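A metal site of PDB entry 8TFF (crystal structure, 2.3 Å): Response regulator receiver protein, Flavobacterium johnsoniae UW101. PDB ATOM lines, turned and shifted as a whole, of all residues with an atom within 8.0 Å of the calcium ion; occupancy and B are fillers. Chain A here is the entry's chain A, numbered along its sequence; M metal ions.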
ATOM      1  N   VAL A 238      34.522  -6.088  33.107  1.00  0.00           N
ATOM      2  CA  VAL A 238      33.873  -7.119  32.318  1.00  0.00           C
ATOM      3  C   VAL A 238      34.084  -6.774  30.842  1.00  0.00           C
ATOM      4  O   VAL A 238      33.493  -5.833  30.334  1.00  0.00           O
ATOM      5  CB  VAL A 238      32.384  -7.195  32.697  1.00  0.00           C
ATOM      6  CG1 VAL A 238      31.650  -8.260  31.912  1.00  0.00           C
ATOM      7  CG2 VAL A 238      32.205  -7.432  34.180  1.00  0.00           C
ATOM      8  N   ILE A 239      34.985  -7.520  30.170  1.00  0.00           N
ATOM      9  CA  ILE A 239      35.091  -7.523  28.728  1.00  0.00           C
ATOM     10  C   ILE A 239      33.942  -8.349  28.155  1.00  0.00           C
ATOM     11  O   ILE A 239      33.786  -9.540  28.418  1.00  0.00           O
ATOM     12  CB  ILE A 239      36.465  -8.045  28.264  1.00  0.00           C
ATOM     13  CG1 ILE A 239      37.605  -7.262  28.889  1.00  0.00           C
ATOM     14  CG2 ILE A 239      36.567  -8.044  26.761  1.00  0.00           C
ATOM     15  CD1 ILE A 239      38.944  -7.862  28.600  1.00  0.00           C
ATOM     16  N   ASP A 240      33.119  -7.683  27.374  1.00  0.00           N
ATOM     17  CA  ASP A 240      31.990  -8.314  26.712  1.00  0.00           C
ATOM     18  C   ASP A 240      32.502  -9.389  25.758  1.00  0.00           C
ATOM     19  O   ASP A 240      33.420  -9.126  24.994  1.00  0.00           O
ATOM     20  CB  ASP A 240      31.180  -7.265  25.966  1.00  0.00           C
ATOM     21  CG  ASP A 240      29.838  -7.758  25.506  1.00  0.00           C
ATOM     22  OD1 ASP A 240      29.075  -8.372  26.334  1.00  0.00           O
ATOM     23  OD2 ASP A 240      29.541  -7.449  24.356  1.00  0.00           O
ATOM     24  N   ASN A 241      31.925 -10.586  25.868  1.00  0.00           N
ATOM     25  CA  ASN A 241      32.057 -11.641  24.896  1.00  0.00           C
ATOM     26  C   ASN A 241      33.462 -12.222  24.804  1.00  0.00           C
ATOM     27  O   ASN A 241      33.774 -12.752  23.763  1.00  0.00           O
ATOM     28  CB  ASN A 241      31.651 -11.168  23.490  1.00  0.00           C
ATOM     29  CG  ASN A 241      30.213 -10.704  23.346  1.00  0.00           C
ATOM     30  OD1 ASN A 241      29.460 -10.620  24.320  1.00  0.00           O
ATOM     31  ND2 ASN A 241      29.831 -10.401  22.123  1.00  0.00           N
ATOM     32  N   LEU A 242      34.266 -12.249  25.859  1.00  0.00           N
ATOM     33  CA  LEU A 242      35.636 -12.759  25.789  1.00  0.00           C
ATOM     34  C   LEU A 242      35.695 -14.272  26.057  1.00  0.00           C
ATOM     35  O   LEU A 242      35.092 -14.750  26.984  1.00  0.00           O
ATOM     36  CB  LEU A 242      36.461 -12.015  26.843  1.00  0.00           C
ATOM     37  CG  LEU A 242      37.969 -12.287  26.801  1.00  0.00           C
ATOM     38  CD1 LEU A 242      38.650 -11.395  25.789  1.00  0.00           C
ATOM     39  CD2 LEU A 242      38.641 -12.094  28.158  1.00  0.00           C
ATOM     40  N   THR A 272      23.864 -17.896  26.593  1.00  0.00           N
ATOM     41  CA  THR A 272      25.205 -17.315  26.721  1.00  0.00           C
ATOM     42  C   THR A 272      25.269 -16.011  25.927  1.00  0.00           C
ATOM     43  O   THR A 272      25.885 -15.957  24.865  1.00  0.00           O
ATOM     44  CB  THR A 272      26.303 -18.285  26.260  1.00  0.00           C
ATOM     45  OG1 THR A 272      25.936 -18.888  25.022  1.00  0.00           O
ATOM     46  CG2 THR A 272      26.537 -19.368  27.303  1.00  0.00           C
ATOM     47  N   ALA A 273      24.563 -15.004  26.462  1.00  0.00           N
ATOM     48  CA  ALA A 273      24.278 -13.759  25.758  1.00  0.00           C
ATOM     49  C   ALA A 273      24.124 -12.616  26.758  1.00  0.00           C
ATOM     50  O   ALA A 273      23.583 -12.788  27.853  1.00  0.00           O
ATOM     51  CB  ALA A 273      23.053 -13.903  24.905  1.00  0.00           C
ATOM     52  N   THR A 274      24.625 -11.441  26.335  1.00  0.00           N
ATOM     53  CA  THR A 274      24.756 -10.243  27.153  1.00  0.00           C
ATOM     54  C   THR A 274      23.481  -9.855  27.928  1.00  0.00           C
ATOM     55  O   THR A 274      23.550  -9.566  29.135  1.00  0.00           O
ATOM     56  CB  THR A 274      25.177  -9.106  26.218  1.00  0.00           C
ATOM     57  OG1 THR A 274      26.190  -9.642  25.348  1.00  0.00           O
ATOM     58  CG2 THR A 274      25.668  -7.897  26.976  1.00  0.00           C
ATOM     59  N   GLN A 275      22.345  -9.807  27.231  1.00  0.00           N
ATOM     60  CA  GLN A 275      21.060  -9.442  27.846  1.00  0.00           C
ATOM     61  C   GLN A 275      20.729 -10.295  29.071  1.00  0.00           C
ATOM     62  O   GLN A 275      20.126  -9.812  30.037  1.00  0.00           O
ATOM     63  CB  GLN A 275      19.967  -9.561  26.786  1.00  0.00           C
ATOM     64  CG  GLN A 275      18.553  -9.420  27.305  1.00  0.00           C
ATOM     65  CD  GLN A 275      17.553  -9.707  26.219  1.00  0.00           C
ATOM     66  OE1 GLN A 275      17.909  -9.872  25.058  1.00  0.00           O
ATOM     67  NE2 GLN A 275      16.278  -9.714  26.566  1.00  0.00           N
ATOM     68  N   TYR A 276      21.124 -11.579  29.057  1.00  0.00           N
ATOM     69  CA  TYR A 276      20.830 -12.460  30.167  1.00  0.00           C
ATOM     70  C   TYR A 276      22.011 -12.524  31.134  1.00  0.00           C
ATOM     71  O   TYR A 276      21.896 -12.131  32.280  1.00  0.00           O
ATOM     72  CB  TYR A 276      20.402 -13.827  29.618  1.00  0.00           C
ATOM     73  CG  TYR A 276      19.135 -13.772  28.815  1.00  0.00           C
ATOM     74  CD1 TYR A 276      19.136 -13.389  27.488  1.00  0.00           C
ATOM     75  CD2 TYR A 276      17.912 -14.006  29.406  1.00  0.00           C
ATOM     76  CE1 TYR A 276      17.967 -13.308  26.753  1.00  0.00           C
ATOM     77  CE2 TYR A 276      16.729 -13.948  28.685  1.00  0.00           C
ATOM     78  CZ  TYR A 276      16.751 -13.558  27.362  1.00  0.00           C
ATOM     79  OH  TYR A 276      15.598 -13.493  26.646  1.00  0.00           O
ATOM     80  N   ALA A 277      23.169 -13.008  30.643  1.00  0.00           N
ATOM     81  CA  ALA A 277      24.298 -13.332  31.505  1.00  0.00           C
ATOM     82  C   ALA A 277      24.922 -12.066  32.096  1.00  0.00           C
ATOM     83  O   ALA A 277      25.367 -12.068  33.239  1.00  0.00           O
ATOM     84  CB  ALA A 277      25.333 -14.120  30.737  1.00  0.00           C
ATOM     85  N   ARG A 278      25.008 -10.994  31.314  1.00  0.00           N
ATOM     86  CA  ARG A 278      25.747  -9.837  31.832  1.00  0.00           C
ATOM     87  C   ARG A 278      24.903  -9.101  32.878  1.00  0.00           C
ATOM     88  O   ARG A 278      25.434  -8.707  33.924  1.00  0.00           O
ATOM     89  CB  ARG A 278      26.220  -8.892  30.725  1.00  0.00           C
ATOM     90  CG  ARG A 278      27.472  -8.149  31.168  1.00  0.00           C
ATOM     91  CD  ARG A 278      28.156  -7.373  30.080  1.00  0.00           C
ATOM     92  NE  ARG A 278      27.386  -6.213  29.724  1.00  0.00           N
ATOM     93  CZ  ARG A 278      27.538  -5.488  28.635  1.00  0.00           C
ATOM     94  NH1 ARG A 278      28.278  -5.939  27.650  1.00  0.00           N
ATOM     95  NH2 ARG A 278      26.957  -4.310  28.563  1.00  0.00           N
ATOM     96  N   ASN A 308      20.913  -3.687  27.781  1.00  0.00           N
ATOM     97  CA  ASN A 308      21.790  -3.618  28.928  1.00  0.00           C
ATOM     98  C   ASN A 308      21.965  -2.162  29.376  1.00  0.00           C
ATOM     99  O   ASN A 308      23.072  -1.724  29.683  1.00  0.00           O
ATOM    100  CB  ASN A 308      23.149  -4.289  28.666  1.00  0.00           C
ATOM    101  CG  ASN A 308      23.040  -5.790  28.557  1.00  0.00           C
ATOM    102  OD1 ASN A 308      22.678  -6.303  27.504  1.00  0.00           O
ATOM    103  ND2 ASN A 308      23.398  -6.497  29.616  1.00  0.00           N
ATOM    104  N   GLU A 311      22.499  -1.683  33.936  1.00  0.00           N
ATOM    105  CA  GLU A 311      23.452  -2.460  34.696  1.00  0.00           C
ATOM    106  C   GLU A 311      23.948  -1.705  35.932  1.00  0.00           C
ATOM    107  O   GLU A 311      24.137  -2.335  36.958  1.00  0.00           O
ATOM    108  CB  GLU A 311      24.600  -2.908  33.790  1.00  0.00           C
ATOM    109  CG  GLU A 311      24.186  -3.882  32.701  1.00  0.00           C
ATOM    110  CD  GLU A 311      25.320  -4.420  31.835  1.00  0.00           C
ATOM    111  OE1 GLU A 311      26.285  -3.663  31.547  1.00  0.00           O
ATOM    112  OE2 GLU A 311      25.205  -5.604  31.434  1.00  0.00           O
ATOM    113  N   VAL A 358      32.440  -2.042  32.037  1.00  0.00           N
ATOM    114  CA  VAL A 358      32.092  -2.894  30.931  1.00  0.00           C
ATOM    115  C   VAL A 358      32.772  -2.350  29.687  1.00  0.00           C
ATOM    116  O   VAL A 358      32.607  -1.167  29.375  1.00  0.00           O
ATOM    117  CB  VAL A 358      30.566  -2.948  30.744  1.00  0.00           C
ATOM    118  CG1 VAL A 358      30.213  -3.762  29.522  1.00  0.00           C
ATOM    119  CG2 VAL A 358      29.885  -3.502  31.986  1.00  0.00           C
ATOM    120  N   ASN A 360      33.232  -3.194  25.738  1.00  0.00           N
ATOM    121  CA  ASN A 360      32.800  -3.944  24.583  1.00  0.00           C
ATOM    122  C   ASN A 360      33.999  -4.221  23.679  1.00  0.00           C
ATOM    123  O   ASN A 360      34.921  -3.425  23.591  1.00  0.00           O
ATOM    124  CB  ASN A 360      31.616  -3.274  23.895  1.00  0.00           C
ATOM    125  CG  ASN A 360      30.358  -3.376  24.728  1.00  0.00           C
ATOM    126  OD1 ASN A 360      30.330  -4.036  25.753  1.00  0.00           O
ATOM    127  ND2 ASN A 360      29.290  -2.736  24.295  1.00  0.00           N
ATOM    128  N   THR A 416      34.365 -11.805  32.206  1.00  0.00           N
ATOM    129  CA  THR A 416      33.523 -11.685  31.033  1.00  0.00           C
ATOM    130  C   THR A 416      32.153 -12.270  31.333  1.00  0.00           C
ATOM    131  O   THR A 416      31.951 -12.838  32.390  1.00  0.00           O
ATOM    132  CB  THR A 416      34.202 -12.381  29.843  1.00  0.00           C
ATOM    133  OG1 THR A 416      33.374 -12.206  28.694  1.00  0.00           O
ATOM    134  CG2 THR A 416      34.477 -13.846  30.125  1.00  0.00           C
ATOM    135  N   ASP A 417      31.206 -12.075  30.413  1.00  0.00           N
ATOM    136  CA  ASP A 417      29.847 -12.578  30.578  1.00  0.00           C
ATOM    137  C   ASP A 417      29.655 -13.936  29.892  1.00  0.00           C
ATOM    138  O   ASP A 417      28.845 -14.708  30.359  1.00  0.00           O
ATOM    139  CB  ASP A 417      28.794 -11.588  30.100  1.00  0.00           C
ATOM    140  CG  ASP A 417      28.979 -11.097  28.674  1.00  0.00           C
ATOM    141  OD1 ASP A 417      30.107 -11.261  28.148  1.00  0.00           O
ATOM    142  OD2 ASP A 417      28.020 -10.555  28.128  1.00  0.00           O
ATOM    143  N   HIS A 418      30.397 -14.198  28.805  1.00  0.00           N
ATOM    144  CA  HIS A 418      30.283 -15.411  27.996  1.00  0.00           C
ATOM    145  C   HIS A 418      31.252 -15.274  26.829  1.00  0.00           C
ATOM    146  O   HIS A 418      31.704 -14.165  26.530  1.00  0.00           O
ATOM    147  CB  HIS A 418      28.837 -15.616  27.496  1.00  0.00           C
ATOM    148  CG  HIS A 418      28.432 -14.508  26.593  1.00  0.00           C
ATOM    149  ND1 HIS A 418      28.849 -14.446  25.274  1.00  0.00           N
ATOM    150  CD2 HIS A 418      27.692 -13.433  26.810  1.00  0.00           C
ATOM    151  CE1 HIS A 418      28.362 -13.326  24.746  1.00  0.00           C
ATOM    152  NE2 HIS A 418      27.721 -12.667  25.685  1.00  0.00           N
ATOM    153  N   GLY A 419      31.597 -16.393  26.217  1.00  0.00           N
ATOM    154  CA  GLY A 419      32.439 -16.402  25.023  1.00  0.00           C
ATOM    155  C   GLY A 419      31.617 -16.536  23.734  1.00  0.00           C
ATOM    156  O   GLY A 419      30.438 -16.262  23.721  1.00  0.00           O
ATOM    157  N   THR A 420      32.306 -16.964  22.676  1.00  0.00           N
ATOM    158  CA  THR A 420      31.779 -17.117  21.345  1.00  0.00           C
ATOM    159  C   THR A 420      32.455 -18.341  20.737  1.00  0.00           C
ATOM    160  O   THR A 420      33.515 -18.794  21.170  1.00  0.00           O
ATOM    161  CB  THR A 420      32.071 -15.924  20.448  1.00  0.00           C
ATOM    162  OG1 THR A 420      33.485 -15.882  20.290  1.00  0.00           O
ATOM    163  CG2 THR A 420      31.589 -14.583  20.959  1.00  0.00           C
ATOM    164  N   HIS A 502      27.357 -16.501  19.696  1.00  0.00           N
ATOM    165  CA  HIS A 502      27.154 -16.847  21.080  1.00  0.00           C
ATOM    166  C   HIS A 502      25.668 -16.989  21.342  1.00  0.00           C
ATOM    167  O   HIS A 502      24.869 -16.590  20.504  1.00  0.00           O
ATOM    168  CB  HIS A 502      27.809 -15.786  21.959  1.00  0.00           C
ATOM    169  CG  HIS A 502      27.229 -14.434  21.761  1.00  0.00           C
ATOM    170  ND1 HIS A 502      26.152 -14.017  22.503  1.00  0.00           N
ATOM    171  CD2 HIS A 502      27.593 -13.393  20.993  1.00  0.00           C
ATOM    172  CE1 HIS A 502      25.864 -12.760  22.193  1.00  0.00           C
ATOM    173  NE2 HIS A 502      26.711 -12.368  21.264  1.00  0.00           N
HETATM  174 CA    CA M   1      28.156 -10.331  25.967  1.00  0.00          CA
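The side-chain amide nitrogen (ND2) of Asn 308 sits at hydrogen-bond distance from the backbone carbonyl oxygen (O) of Thr 274 (3.1 Å).
The side-chain carboxylate (OD1) of Asp 417 is in hydrogen-bond range of the side-chain hydroxyl (OG1) of Thr 416.
OD2 of Asp 240 lies within salt-bridge range of NH1 of Arg 278, at 3.8 Å.
A ring nitrogen (ND1) of His 418 lies within hydrogen-bond range of the backbone carbonyl oxygen of Thr 272 (3.4 Å).
OG1 of Thr 416 is in hydrogen-bond range of O of His 418, 3.4 Å away.
N of Leu 242 sits at hydrogen-bond distance from O of His 418 (3.3 Å).
The calcium ion is bound by the side-chain amide oxygen of Asn 241 (2.1 Å), the side-chain hydroxyl of Thr 274 (2.2 Å), the side-chain carboxylate of Asp 417 (2.2 Å), the side-chain carboxylate of Asp 240 (2.2 Å) and a ring nitrogen (NE2) of His 418 (2.4 Å).
Slightly farther from the calcium ion lies OD1 of Asp 417 (3.1 Å).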
